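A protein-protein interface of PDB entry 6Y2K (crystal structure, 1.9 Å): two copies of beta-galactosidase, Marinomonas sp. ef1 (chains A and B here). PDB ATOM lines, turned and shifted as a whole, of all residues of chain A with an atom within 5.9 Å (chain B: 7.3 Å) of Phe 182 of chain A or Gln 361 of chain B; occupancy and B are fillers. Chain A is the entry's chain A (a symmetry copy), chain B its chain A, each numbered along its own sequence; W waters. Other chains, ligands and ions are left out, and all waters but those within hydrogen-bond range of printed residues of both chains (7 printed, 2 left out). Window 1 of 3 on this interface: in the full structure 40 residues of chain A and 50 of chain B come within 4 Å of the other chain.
The backbone carbonyl oxygen of Glu 202 of chain A lies within hydrogen-bond range of the side-chain amide nitrogen of Gln 361 of chain B.
The backbone carbonyl oxygen of Phe 37 of chain B is in hydrogen-bond range of the side-chain hydroxyl of Ser 184 of chain A (2.6 Å).
The side-chain sulfur (SD) of Met 185 of chain A sits at hydrogen-bond distance from the side-chain amide nitrogen (NE2) of Gln 361 of chain B (3.7 Å).
The side-chain carboxylate (OD2) of Asp 186 of chain A lies within hydrogen-bond range of the side-chain hydroxyl (OG) of Ser 40 of chain B, 2.6 Å away.
NE2 of Gln 361 of chain B lies close to N of Asn 204 of chain A (3.2 Å).
O of Gln 361 of chain B is in hydrogen-bond range of NE2 of Gln 427 of chain A, at 2.9 Å.
SD of Met 185 of chain A lies close to O of Gly 101 of chain B (3.5 Å).
The side-chain hydroxyl of Ser 184 of chain A sits at hydrogen-bond distance from the backbone NH of Ser 40 of chain B (2.9 Å).
O of Asn 180 of chain A lies within hydrogen-bond range of N of Met 185 of chain A, at 2.8 Å.
The side-chain amide oxygen of Asn 180 of chain A sits at hydrogen-bond distance from the side-chain amide nitrogen of Asn 204 of chain A (3.1 Å).
Among the printed residues, pairs that only touch across the chains: Glu 202 of chain A with Ser 102 of chain B, Phe 182 of chain A with Gln 361 of chain B, Ser 184 of chain A with Thr 76 of chain B, Ala 203 of chain A with Gln 361 of chain B, Trp 183 of chain A with Arg 103 of chain B, Trp 183 of chain A with Thr 76 of chain B, Trp 183 of chain A with Gln 361 of chain B, Trp 183 of chain A with Glu 362 of chain B, Gly 179 of chain A with Phe 359 of chain B, Ala 203 of chain A with Gly 101 of chain B, Phe 182 of chain A with Glu 362 of chain B, Pro 205 of chain A with Gly 360 of chain B, Trp 183 of chain A with Ser 102 of chain B, Val 181 of chain A with Thr 41 of chain B, Val 181 of chain A with His 11 of chain B, Pro 205 of chain A with Gln 361 of chain B, Val 181 of chain A with Phe 359 of chain B, Val 181 of chain A with Glu 10 of chain B, Asn 204 of chain A with Gly 101 of chain B, Asn 204 of chain A with Gly 360 of chain B, Phe 182 of chain A with His 11 of chain B, Trp 183 of chain A with Phe 37 of chain B and Pro 205 of chain A with Gln 363 of chain B.
Of the printed residues of chain B, Gly 179 of chain A touches Phe 359.
Of chain B, only His 11 (3.9 Å), Gln 361 (3.3 Å) and Glu 362 (3.6 Å) come within 4 Å of Phe 182 of chain A.
Printed residues of chain B within 4 Å of Met 185 of chain A: Gly 101 and Gln 361.
Printed residues of chain B within 4 Å of Asp 186 of chain A: Ser 40 (2.6 Å).
Of the printed residues of chain A, Ser 102 of chain B touches Trp 183 (3.7 Å) and Glu 202 (3.2 Å).
Of chain A, only Phe 182 (3.3 Å), Trp 183 (3.5 Å), Met 185 (3.4 Å), Glu 202 (2.9 Å), Ala 203 (3.3 Å), Asn 204 (3.2 Å), Pro 205 (3.7 Å) and Gln 427 (2.9 Å) come within 4 Å of Gln 361 of chain B.
The nearest printed residue of chain B that does not touch Glu 202 of chain A is Gly 101 of chain B (4.2 Å).
Among the printed residues, 31 pairs touch across the chains.
No position is printed for both chains.
Of the 31 pairs that touch across the chains among the printed residues, none has its exchanged pair printed and touching as well.
Water W5 lies within hydrogen-bond range of OE2 of Glu 362 of chain B and NE1 of Trp 183 of chain A.
Water W7 bridges N of Trp 183 of chain A (3.0 Å) and NE2 of His 11 of chain B (3.3 Å).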
ATOM      1  N   GLY A 179      -9.180  19.448   4.574  1.00  0.00           N
ATOM      2  CA  GLY A 179      -9.860  18.565   3.625  1.00  0.00           C
ATOM      3  C   GLY A 179      -8.951  17.493   3.025  1.00  0.00           C
ATOM      4  O   GLY A 179      -9.057  17.169   1.836  1.00  0.00           O
ATOM      5  N   ASN A 180      -8.096  16.902   3.864  1.00  0.00           N
ATOM      6  CA  ASN A 180      -7.046  15.986   3.396  1.00  0.00           C
ATOM      7  C   ASN A 180      -7.547  14.613   2.935  1.00  0.00           C
ATOM      8  O   ASN A 180      -6.745  13.797   2.462  1.00  0.00           O
ATOM      9  CB  ASN A 180      -5.941  15.834   4.452  1.00  0.00           C
ATOM     10  CG  ASN A 180      -5.033  17.053   4.534  1.00  0.00           C
ATOM     11  OD1 ASN A 180      -4.914  17.829   3.571  1.00  0.00           O
ATOM     12  ND2 ASN A 180      -4.374  17.227   5.687  1.00  0.00           N
ATOM     13  N   VAL A 181      -8.852  14.355   3.048  1.00  0.00           N
ATOM     14  CA  VAL A 181      -9.462  13.224   2.333  1.00  0.00           C
ATOM     15  C   VAL A 181      -9.209  13.320   0.818  1.00  0.00           C
ATOM     16  O   VAL A 181      -9.019  12.299   0.135  1.00  0.00           O
ATOM     17  CB  VAL A 181     -10.978  13.107   2.636  1.00  0.00           C
ATOM     18  CG1 VAL A 181     -11.761  14.298   2.087  1.00  0.00           C
ATOM     19  CG2 VAL A 181     -11.529  11.791   2.088  1.00  0.00           C
ATOM     20  N   PHE A 182      -9.187  14.554   0.312  1.00  0.00           N
ATOM     21  CA  PHE A 182      -8.885  14.842  -1.088  1.00  0.00           C
ATOM     22  C   PHE A 182      -7.479  14.353  -1.467  1.00  0.00           C
ATOM     23  O   PHE A 182      -6.502  14.610  -0.751  1.00  0.00           O
ATOM     24  CB  PHE A 182      -9.026  16.355  -1.336  1.00  0.00           C
ATOM     25  CG  PHE A 182      -8.945  16.752  -2.781  1.00  0.00           C
ATOM     26  CD1 PHE A 182     -10.017  16.528  -3.636  1.00  0.00           C
ATOM     27  CD2 PHE A 182      -7.799  17.362  -3.286  1.00  0.00           C
ATOM     28  CE1 PHE A 182      -9.949  16.883  -4.975  1.00  0.00           C
ATOM     29  CE2 PHE A 182      -7.726  17.740  -4.621  1.00  0.00           C
ATOM     30  CZ  PHE A 182      -8.804  17.503  -5.467  1.00  0.00           C
ATOM     31  N   TRP A 183      -7.398  13.617  -2.575  1.00  0.00           N
ATOM     32  CA  TRP A 183      -6.152  13.012  -3.051  1.00  0.00           C
ATOM     33  C   TRP A 183      -5.373  12.220  -1.985  1.00  0.00           C
ATOM     34  O   TRP A 183      -4.144  12.161  -2.019  1.00  0.00           O
ATOM     35  CB  TRP A 183      -5.242  14.080  -3.706  1.00  0.00           C
ATOM     36  CG  TRP A 183      -5.784  14.700  -4.966  1.00  0.00           C
ATOM     37  CD1 TRP A 183      -6.868  14.290  -5.693  1.00  0.00           C
ATOM     38  CD2 TRP A 183      -5.226  15.817  -5.678  1.00  0.00           C
ATOM     39  NE1 TRP A 183      -7.034  15.101  -6.794  1.00  0.00           N
ATOM     40  CE2 TRP A 183      -6.042  16.043  -6.811  1.00  0.00           C
ATOM     41  CE3 TRP A 183      -4.135  16.664  -5.453  1.00  0.00           C
ATOM     42  CZ2 TRP A 183      -5.804  17.076  -7.709  1.00  0.00           C
ATOM     43  CZ3 TRP A 183      -3.890  17.686  -6.355  1.00  0.00           C
ATOM     44  CH2 TRP A 183      -4.724  17.885  -7.468  1.00  0.00           C
ATOM     45  N   SER A 184      -6.091  11.593  -1.053  1.00  0.00           N
ATOM     46  CA  SER A 184      -5.474  10.806   0.033  1.00  0.00           C
ATOM     47  C   SER A 184      -4.289  11.521   0.714  1.00  0.00           C
ATOM     48  O   SER A 184      -3.206  10.951   0.903  1.00  0.00           O
ATOM     49  CB  SER A 184      -5.075   9.424  -0.497  1.00  0.00           C
ATOM     50  OG  SER A 184      -6.216   8.590  -0.676  1.00  0.00           O
ATOM     51  N   MET A 185      -4.507  12.780   1.071  1.00  0.00           N
ATOM     52  CA  MET A 185      -3.468  13.589   1.722  1.00  0.00           C
ATOM     53  C   MET A 185      -3.375  13.363   3.251  1.00  0.00           C
ATOM     54  O   MET A 185      -2.445  13.874   3.889  1.00  0.00           O
ATOM     55  CB  MET A 185      -3.683  15.080   1.419  1.00  0.00           C
ATOM     56  CG  MET A 185      -3.297  15.499  -0.003  1.00  0.00           C
ATOM     57  SD  MET A 185      -3.425  17.279  -0.336  1.00  0.00           S
ATOM     58  CE  MET A 185      -5.198  17.536  -0.282  1.00  0.00           C
ATOM     59  N   ASP A 186      -4.322  12.618   3.828  1.00  0.00           N
ATOM     60  CA  ASP A 186      -4.441  12.465   5.297  1.00  0.00           C
ATOM     61  C   ASP A 186      -3.131  12.090   5.993  1.00  0.00           C
ATOM     62  O   ASP A 186      -2.462  11.133   5.595  1.00  0.00           O
ATOM     63  CB  ASP A 186      -5.496  11.409   5.655  1.00  0.00           C
ATOM     64  CG  ASP A 186      -6.919  11.859   5.341  1.00  0.00           C
ATOM     65  OD1 ASP A 186      -7.320  12.955   5.807  1.00  0.00           O
ATOM     66  OD2 ASP A 186      -7.629  11.098   4.631  1.00  0.00           O
ATOM     67  N   GLU A 202       0.376  20.980  -7.717  1.00  0.00           N
ATOM     68  CA  GLU A 202      -0.187  21.918  -6.719  1.00  0.00           C
ATOM     69  C   GLU A 202      -0.443  21.300  -5.330  1.00  0.00           C
ATOM     70  O   GLU A 202      -1.192  20.326  -5.208  1.00  0.00           O
ATOM     71  CB  GLU A 202      -1.490  22.536  -7.233  1.00  0.00           C
ATOM     72  CG  GLU A 202      -1.977  23.710  -6.390  1.00  0.00           C
ATOM     73  CD  GLU A 202      -3.310  24.285  -6.831  1.00  0.00           C
ATOM     74  OE1 GLU A 202      -4.020  23.654  -7.658  1.00  0.00           O
ATOM     75  OE2 GLU A 202      -3.651  25.376  -6.314  1.00  0.00           O
ATOM     76  N   ALA A 203       0.148  21.911  -4.299  1.00  0.00           N
ATOM     77  CA  ALA A 203      -0.092  21.523  -2.903  1.00  0.00           C
ATOM     78  C   ALA A 203      -1.456  22.048  -2.444  1.00  0.00           C
ATOM     79  O   ALA A 203      -2.033  22.940  -3.068  1.00  0.00           O
ATOM     80  CB  ALA A 203       1.017  22.058  -1.993  1.00  0.00           C
ATOM     81  N   ASN A 204      -1.967  21.489  -1.354  1.00  0.00           N
ATOM     82  CA  ASN A 204      -3.273  21.888  -0.821  1.00  0.00           C
ATOM     83  C   ASN A 204      -3.203  23.384  -0.492  1.00  0.00           C
ATOM     84  O   ASN A 204      -2.260  23.806   0.174  1.00  0.00           O
ATOM     85  CB  ASN A 204      -3.590  21.075   0.442  1.00  0.00           C
ATOM     86  CG  ASN A 204      -5.016  21.271   0.956  1.00  0.00           C
ATOM     87  OD1 ASN A 204      -5.692  22.250   0.628  1.00  0.00           O
ATOM     88  ND2 ASN A 204      -5.467  20.336   1.794  1.00  0.00           N
ATOM     89  N   PRO A 205      -4.178  24.192  -0.972  1.00  0.00           N
ATOM     90  CA  PRO A 205      -4.134  25.606  -0.584  1.00  0.00           C
ATOM     91  C   PRO A 205      -4.177  25.863   0.936  1.00  0.00           C
ATOM     92  O   PRO A 205      -3.634  26.878   1.385  1.00  0.00           O
ATOM     93  CB  PRO A 205      -5.357  26.212  -1.294  1.00  0.00           C
ATOM     94  CG  PRO A 205      -6.226  25.045  -1.658  1.00  0.00           C
ATOM     95  CD  PRO A 205      -5.259  23.937  -1.947  1.00  0.00           C
ATOM     96  N   GLN A 427      -4.388  30.881  -4.796  1.00  0.00           N
ATOM     97  CA  GLN A 427      -5.222  30.503  -5.956  1.00  0.00           C
ATOM     98  C   GLN A 427      -5.892  31.752  -6.532  1.00  0.00           C
ATOM     99  O   GLN A 427      -7.014  32.105  -6.138  1.00  0.00           O
ATOM    100  CB  GLN A 427      -6.278  29.451  -5.588  1.00  0.00           C
ATOM    101  CG  GLN A 427      -5.700  28.081  -5.261  1.00  0.00           C
ATOM    102  CD  GLN A 427      -6.739  26.965  -5.294  1.00  0.00           C
ATOM    103  OE1 GLN A 427      -7.938  27.204  -5.096  1.00  0.00           O
ATOM    104  NE2 GLN A 427      -6.283  25.734  -5.552  1.00  0.00           N
ATOM    105  N   TYR B   8     -17.578  11.157  -5.486  1.00  0.00           N
ATOM    106  CA  TYR B   8     -16.721  10.991  -4.297  1.00  0.00           C
ATOM    107  C   TYR B   8     -17.578  10.863  -3.035  1.00  0.00           C
ATOM    108  O   TYR B   8     -17.698  11.805  -2.263  1.00  0.00           O
ATOM    109  CB  TYR B   8     -15.696  12.135  -4.231  1.00  0.00           C
ATOM    110  CG  TYR B   8     -14.853  12.087  -5.490  1.00  0.00           C
ATOM    111  CD1 TYR B   8     -15.271  12.746  -6.651  1.00  0.00           C
ATOM    112  CD2 TYR B   8     -13.728  11.282  -5.560  1.00  0.00           C
ATOM    113  CE1 TYR B   8     -14.554  12.653  -7.826  1.00  0.00           C
ATOM    114  CE2 TYR B   8     -12.995  11.185  -6.733  1.00  0.00           C
ATOM    115  CZ  TYR B   8     -13.420  11.877  -7.861  1.00  0.00           C
ATOM    116  OH  TYR B   8     -12.723  11.781  -9.021  1.00  0.00           O
ATOM    117  N   GLU B  10     -16.912   9.424  -0.332  1.00  0.00           N
ATOM    118  CA  GLU B  10     -16.023   9.720   0.794  1.00  0.00           C
ATOM    119  C   GLU B  10     -15.831  11.221   1.116  1.00  0.00           C
ATOM    120  O   GLU B  10     -15.295  11.559   2.185  1.00  0.00           O
ATOM    121  CB  GLU B  10     -14.660   9.005   0.623  1.00  0.00           C
ATOM    122  CG  GLU B  10     -13.659   9.643  -0.343  1.00  0.00           C
ATOM    123  CD  GLU B  10     -13.795   9.221  -1.797  1.00  0.00           C
ATOM    124  OE1 GLU B  10     -14.899   8.803  -2.252  1.00  0.00           O
ATOM    125  OE2 GLU B  10     -12.765   9.333  -2.500  1.00  0.00           O
ATOM    126  N   HIS B  11     -16.236  12.116   0.213  1.00  0.00           N
ATOM    127  CA  HIS B  11     -16.215  13.561   0.492  1.00  0.00           C
ATOM    128  C   HIS B  11     -17.479  14.111   1.147  1.00  0.00           C
ATOM    129  O   HIS B  11     -17.495  15.285   1.534  1.00  0.00           O
ATOM    130  CB  HIS B  11     -15.942  14.343  -0.791  1.00  0.00           C
ATOM    131  CG  HIS B  11     -14.605  14.056  -1.398  1.00  0.00           C
ATOM    132  ND1 HIS B  11     -14.208  14.591  -2.601  1.00  0.00           N
ATOM    133  CD2 HIS B  11     -13.579  13.280  -0.975  1.00  0.00           C
ATOM    134  CE1 HIS B  11     -13.001  14.148  -2.901  1.00  0.00           C
ATOM    135  NE2 HIS B  11     -12.592  13.356  -1.926  1.00  0.00           N
ATOM    136  N   PHE B  37      -9.152   7.888  -5.572  1.00  0.00           N
ATOM    137  CA  PHE B  37      -8.339   8.676  -4.633  1.00  0.00           C
ATOM    138  C   PHE B  37      -8.555   8.305  -3.158  1.00  0.00           C
ATOM    139  O   PHE B  37      -8.229   9.102  -2.269  1.00  0.00           O
ATOM    140  CB  PHE B  37      -8.603  10.180  -4.827  1.00  0.00           C
ATOM    141  CG  PHE B  37      -8.281  10.696  -6.212  1.00  0.00           C
ATOM    142  CD1 PHE B  37      -7.026  10.502  -6.773  1.00  0.00           C
ATOM    143  CD2 PHE B  37      -9.217  11.435  -6.924  1.00  0.00           C
ATOM    144  CE1 PHE B  37      -6.722  10.993  -8.039  1.00  0.00           C
ATOM    145  CE2 PHE B  37      -8.912  11.946  -8.176  1.00  0.00           C
ATOM    146  CZ  PHE B  37      -7.666  11.724  -8.736  1.00  0.00           C
ATOM    147  N   SER B  40      -6.174   6.682   1.470  1.00  0.00           N
ATOM    148  CA  SER B  40      -6.101   7.148   2.872  1.00  0.00           C
ATOM    149  C   SER B  40      -7.390   6.882   3.674  1.00  0.00           C
ATOM    150  O   SER B  40      -7.333   6.803   4.898  1.00  0.00           O
ATOM    151  CB  SER B  40      -5.700   8.627   2.984  1.00  0.00           C
ATOM    152  OG  SER B  40      -6.791   9.511   2.769  1.00  0.00           O
ATOM    153  N   THR B  41      -8.531   6.750   2.994  1.00  0.00           N
ATOM    154  CA  THR B  41      -9.790   6.350   3.646  1.00  0.00           C
ATOM    155  C   THR B  41      -9.783   4.835   3.909  1.00  0.00           C
ATOM    156  O   THR B  41     -10.173   4.389   4.990  1.00  0.00           O
ATOM    157  CB  THR B  41     -11.012   6.756   2.793  1.00  0.00           C
ATOM    158  OG1 THR B  41     -11.007   8.178   2.592  1.00  0.00           O
ATOM    159  CG2 THR B  41     -12.324   6.359   3.464  1.00  0.00           C
ATOM    160  N   THR B  76      -2.630   7.992  -5.838  1.00  0.00           N
ATOM    161  CA  THR B  76      -2.418   8.787  -4.636  1.00  0.00           C
ATOM    162  C   THR B  76      -2.197   7.890  -3.409  1.00  0.00           C
ATOM    163  O   THR B  76      -3.069   7.794  -2.546  1.00  0.00           O
ATOM    164  CB  THR B  76      -3.606   9.751  -4.399  1.00  0.00           C
ATOM    165  OG1 THR B  76      -4.848   9.080  -4.625  1.00  0.00           O
ATOM    166  CG2 THR B  76      -3.527  10.929  -5.343  1.00  0.00           C
ATOM    167  N   GLY B 101       2.161  15.493  -1.124  1.00  0.00           N
ATOM    168  CA  GLY B 101       1.418  16.724  -0.859  1.00  0.00           C
ATOM    169  C   GLY B 101       0.455  17.140  -1.960  1.00  0.00           C
ATOM    170  O   GLY B 101      -0.319  18.096  -1.774  1.00  0.00           O
ATOM    171  N   SER B 102       0.531  16.449  -3.108  1.00  0.00           N
ATOM    172  CA  SER B 102      -0.370  16.640  -4.236  1.00  0.00           C
ATOM    173  C   SER B 102      -0.831  15.239  -4.679  1.00  0.00           C
ATOM    174  O   SER B 102      -1.451  14.523  -3.869  1.00  0.00           O
ATOM    175  CB  SER B 102       0.318  17.469  -5.351  1.00  0.00           C
ATOM    176  OG  SER B 102       1.432  16.797  -5.938  1.00  0.00           O
ATOM    177  N   ARG B 103      -0.544  14.841  -5.915  1.00  0.00           N
ATOM    178  CA  ARG B 103      -0.877  13.493  -6.397  1.00  0.00           C
ATOM    179  C   ARG B 103       0.190  13.001  -7.366  1.00  0.00           C
ATOM    180  O   ARG B 103       1.045  13.779  -7.786  1.00  0.00           O
ATOM    181  CB  ARG B 103      -2.267  13.467  -7.067  1.00  0.00           C
ATOM    182  CG  ARG B 103      -2.451  14.425  -8.243  1.00  0.00           C
ATOM    183  CD  ARG B 103      -3.803  14.221  -8.922  1.00  0.00           C
ATOM    184  NE  ARG B 103      -4.045  15.198  -9.985  1.00  0.00           N
ATOM    185  CZ  ARG B 103      -5.214  15.384 -10.607  1.00  0.00           C
ATOM    186  NH1 ARG B 103      -6.306  14.677 -10.288  1.00  0.00           N
ATOM    187  NH2 ARG B 103      -5.295  16.306 -11.561  1.00  0.00           N
ATOM    188  N   ASN B 321     -10.364  24.673 -12.515  1.00  0.00           N
ATOM    189  CA  ASN B 321      -9.453  25.394 -11.604  1.00  0.00           C
ATOM    190  C   ASN B 321      -8.029  25.570 -12.130  1.00  0.00           C
ATOM    191  O   ASN B 321      -7.308  26.431 -11.631  1.00  0.00           O
ATOM    192  CB  ASN B 321      -9.322  24.633 -10.282  1.00  0.00           C
ATOM    193  CG  ASN B 321      -8.770  23.230 -10.479  1.00  0.00           C
ATOM    194  OD1 ASN B 321      -9.460  22.377 -11.040  1.00  0.00           O
ATOM    195  ND2 ASN B 321      -7.513  22.995 -10.072  1.00  0.00           N
ATOM    196  N   TRP B 322      -7.621  24.746 -13.095  1.00  0.00           N
ATOM    197  CA  TRP B 322      -6.188  24.482 -13.332  1.00  0.00           C
ATOM    198  C   TRP B 322      -5.532  25.241 -14.487  1.00  0.00           C
ATOM    199  O   TRP B 322      -4.309  25.293 -14.549  1.00  0.00           O
ATOM    200  CB  TRP B 322      -5.910  22.974 -13.452  1.00  0.00           C
ATOM    201  CG  TRP B 322      -6.803  22.210 -14.391  1.00  0.00           C
ATOM    202  CD1 TRP B 322      -7.859  21.416 -14.045  1.00  0.00           C
ATOM    203  CD2 TRP B 322      -6.709  22.152 -15.817  1.00  0.00           C
ATOM    204  NE1 TRP B 322      -8.434  20.878 -15.166  1.00  0.00           N
ATOM    205  CE2 TRP B 322      -7.743  21.305 -16.268  1.00  0.00           C
ATOM    206  CE3 TRP B 322      -5.851  22.733 -16.762  1.00  0.00           C
ATOM    207  CZ2 TRP B 322      -7.949  21.032 -17.618  1.00  0.00           C
ATOM    208  CZ3 TRP B 322      -6.053  22.449 -18.114  1.00  0.00           C
ATOM    209  CH2 TRP B 322      -7.097  21.612 -18.527  1.00  0.00           C
ATOM    210  N   PHE B 352     -17.546  15.287 -14.537  1.00  0.00           N
ATOM    211  CA  PHE B 352     -16.702  15.344 -13.350  1.00  0.00           C
ATOM    212  C   PHE B 352     -16.588  16.771 -12.823  1.00  0.00           C
ATOM    213  O   PHE B 352     -16.131  17.669 -13.530  1.00  0.00           O
ATOM    214  CB  PHE B 352     -15.312  14.783 -13.653  1.00  0.00           C
ATOM    215  CG  PHE B 352     -14.288  15.100 -12.602  1.00  0.00           C
ATOM    216  CD1 PHE B 352     -13.780  16.383 -12.474  1.00  0.00           C
ATOM    217  CD2 PHE B 352     -13.832  14.116 -11.739  1.00  0.00           C
ATOM    218  CE1 PHE B 352     -12.838  16.677 -11.508  1.00  0.00           C
ATOM    219  CE2 PHE B 352     -12.890  14.404 -10.770  1.00  0.00           C
ATOM    220  CZ  PHE B 352     -12.392  15.687 -10.654  1.00  0.00           C
ATOM    221  N   ARG B 353     -17.006  16.971 -11.578  1.00  0.00           N
ATOM    222  CA  ARG B 353     -17.541  15.885 -10.765  1.00  0.00           C
ATOM    223  C   ARG B 353     -19.039  16.055 -10.533  1.00  0.00           C
ATOM    224  O   ARG B 353     -19.665  16.958 -11.088  1.00  0.00           O
ATOM    225  CB  ARG B 353     -16.808  15.808  -9.425  1.00  0.00           C
ATOM    226  CG  ARG B 353     -16.223  17.131  -8.960  1.00  0.00           C
ATOM    227  CD  ARG B 353     -15.257  16.933  -7.803  1.00  0.00           C
ATOM    228  NE  ARG B 353     -15.932  16.439  -6.606  1.00  0.00           N
ATOM    229  CZ  ARG B 353     -15.310  16.130  -5.473  1.00  0.00           C
ATOM    230  NH1 ARG B 353     -13.995  16.263  -5.377  1.00  0.00           N
ATOM    231  NH2 ARG B 353     -16.005  15.686  -4.434  1.00  0.00           N
ATOM    232  N   ALA B 357     -16.473  20.303  -4.824  1.00  0.00           N
ATOM    233  CA  ALA B 357     -15.984  20.126  -3.449  1.00  0.00           C
ATOM    234  C   ALA B 357     -15.655  21.484  -2.829  1.00  0.00           C
ATOM    235  O   ALA B 357     -15.137  22.349  -3.520  1.00  0.00           O
ATOM    236  CB  ALA B 357     -14.759  19.228  -3.439  1.00  0.00           C
ATOM    237  N   PHE B 359     -13.424  21.994  -0.452  1.00  0.00           N
ATOM    238  CA  PHE B 359     -12.058  21.927   0.086  1.00  0.00           C
ATOM    239  C   PHE B 359     -11.071  21.424  -0.970  1.00  0.00           C
ATOM    240  O   PHE B 359     -11.471  20.871  -1.998  1.00  0.00           O
ATOM    241  CB  PHE B 359     -11.995  21.008   1.330  1.00  0.00           C
ATOM    242  CG  PHE B 359     -12.661  19.672   1.134  1.00  0.00           C
ATOM    243  CD1 PHE B 359     -12.027  18.652   0.433  1.00  0.00           C
ATOM    244  CD2 PHE B 359     -13.951  19.453   1.614  1.00  0.00           C
ATOM    245  CE1 PHE B 359     -12.652  17.436   0.229  1.00  0.00           C
ATOM    246  CE2 PHE B 359     -14.577  18.233   1.422  1.00  0.00           C
ATOM    247  CZ  PHE B 359     -13.925  17.225   0.722  1.00  0.00           C
ATOM    248  N   GLY B 360      -9.782  21.615  -0.687  1.00  0.00           N
ATOM    249  CA  GLY B 360      -8.695  21.076  -1.513  1.00  0.00           C
ATOM    250  C   GLY B 360      -8.361  21.888  -2.752  1.00  0.00           C
ATOM    251  O   GLY B 360      -8.946  22.961  -2.993  1.00  0.00           O
ATOM    252  N   GLN B 361      -7.424  21.353  -3.543  1.00  0.00           N
ATOM    253  CA  GLN B 361      -6.845  22.030  -4.719  1.00  0.00           C
ATOM    254  C   GLN B 361      -7.890  22.422  -5.776  1.00  0.00           C
ATOM    255  O   GLN B 361      -7.745  23.441  -6.462  1.00  0.00           O
ATOM    256  CB  GLN B 361      -5.779  21.128  -5.388  1.00  0.00           C
ATOM    257  CG  GLN B 361      -4.441  21.002  -4.666  1.00  0.00           C
ATOM    258  CD  GLN B 361      -4.378  19.915  -3.583  1.00  0.00           C
ATOM    259  OE1 GLN B 361      -5.389  19.581  -2.949  1.00  0.00           O
ATOM    260  NE2 GLN B 361      -3.178  19.371  -3.360  1.00  0.00           N
ATOM    261  N   GLU B 362      -8.926  21.597  -5.912  1.00  0.00           N
ATOM    262  CA  GLU B 362      -9.950  21.748  -6.948  1.00  0.00           C
ATOM    263  C   GLU B 362     -11.276  22.290  -6.410  1.00  0.00           C
ATOM    264  O   GLU B 362     -12.324  22.082  -7.023  1.00  0.00           O
ATOM    265  CB  GLU B 362     -10.153  20.402  -7.662  1.00  0.00           C
ATOM    266  CG  GLU B 362      -8.932  19.977  -8.466  1.00  0.00           C
ATOM    267  CD  GLU B 362      -9.067  18.630  -9.152  1.00  0.00           C
ATOM    268  OE1 GLU B 362      -8.180  18.319  -9.985  1.00  0.00           O
ATOM    269  OE2 GLU B 362     -10.038  17.883  -8.866  1.00  0.00           O
ATOM    270  N   GLN B 363     -11.243  23.023  -5.298  1.00  0.00           N
ATOM    271  CA  GLN B 363     -12.472  23.619  -4.764  1.00  0.00           C
ATOM    272  C   GLN B 363     -13.190  24.586  -5.747  1.00  0.00           C
ATOM    273  O   GLN B 363     -14.403  24.780  -5.635  1.00  0.00           O
ATOM    274  CB  GLN B 363     -12.240  24.267  -3.383  1.00  0.00           C
ATOM    275  CG  GLN B 363     -11.358  25.510  -3.366  1.00  0.00           C
ATOM    276  CD  GLN B 363     -10.946  25.919  -1.960  1.00  0.00           C
ATOM    277  OE1 GLN B 363     -11.359  26.972  -1.465  1.00  0.00           O
ATOM    278  NE2 GLN B 363     -10.133  25.078  -1.301  1.00  0.00           N
ATOM    279  N   MET B 364     -12.458  25.157  -6.712  1.00  0.00           N
ATOM    280  CA  MET B 364     -13.067  25.985  -7.772  1.00  0.00           C
ATOM    281  C   MET B 364     -13.440  25.220  -9.058  1.00  0.00           C
ATOM    282  O   MET B 364     -13.879  25.844 -10.028  1.00  0.00           O
ATOM    283  CB  MET B 364     -12.146  27.164  -8.127  1.00  0.00           C
ATOM    284  CG  MET B 364     -11.799  28.072  -6.957  1.00  0.00           C
ATOM    285  SD  MET B 364     -13.239  28.797  -6.151  1.00  0.00           S
ATOM    286  CE  MET B 364     -13.782  29.960  -7.390  1.00  0.00           C
ATOM    287  N   HIS B 365     -13.300  23.892  -9.066  1.00  0.00           N
ATOM    288  CA  HIS B 365     -13.679  23.071 -10.224  1.00  0.00           C
ATOM    289  C   HIS B 365     -15.169  22.739 -10.123  1.00  0.00           C
ATOM    290  O   HIS B 365     -15.589  22.081  -9.180  1.00  0.00           O
ATOM    291  CB  HIS B 365     -12.856  21.780 -10.270  1.00  0.00           C
ATOM    292  CG  HIS B 365     -12.957  21.028 -11.562  1.00  0.00           C
ATOM    293  ND1 HIS B 365     -14.160  20.601 -12.091  1.00  0.00           N
ATOM    294  CD2 HIS B 365     -11.996  20.581 -12.409  1.00  0.00           C
ATOM    295  CE1 HIS B 365     -13.935  19.948 -13.218  1.00  0.00           C
ATOM    296  NE2 HIS B 365     -12.630  19.909 -13.426  1.00  0.00           N
HETATM  297  O   HOH W   1      -9.437  25.493  -6.888  1.00  0.00           O
HETATM  298  O   HOH W   2      -0.565  19.605   0.435  1.00  0.00           O
HETATM  299  O   HOH W   3      -9.052   9.330   1.139  1.00  0.00           O
HETATM  300  O   HOH W   4      -5.529   6.920  -3.205  1.00  0.00           O
HETATM  301  O   HOH W   5      -9.642  15.308  -8.303  1.00  0.00           O
HETATM  302  O   HOH W   6      -5.831  25.028  -8.958  1.00  0.00           O
HETATM  303  O   HOH W   7     -10.011  13.199  -3.947  1.00  0.00           O
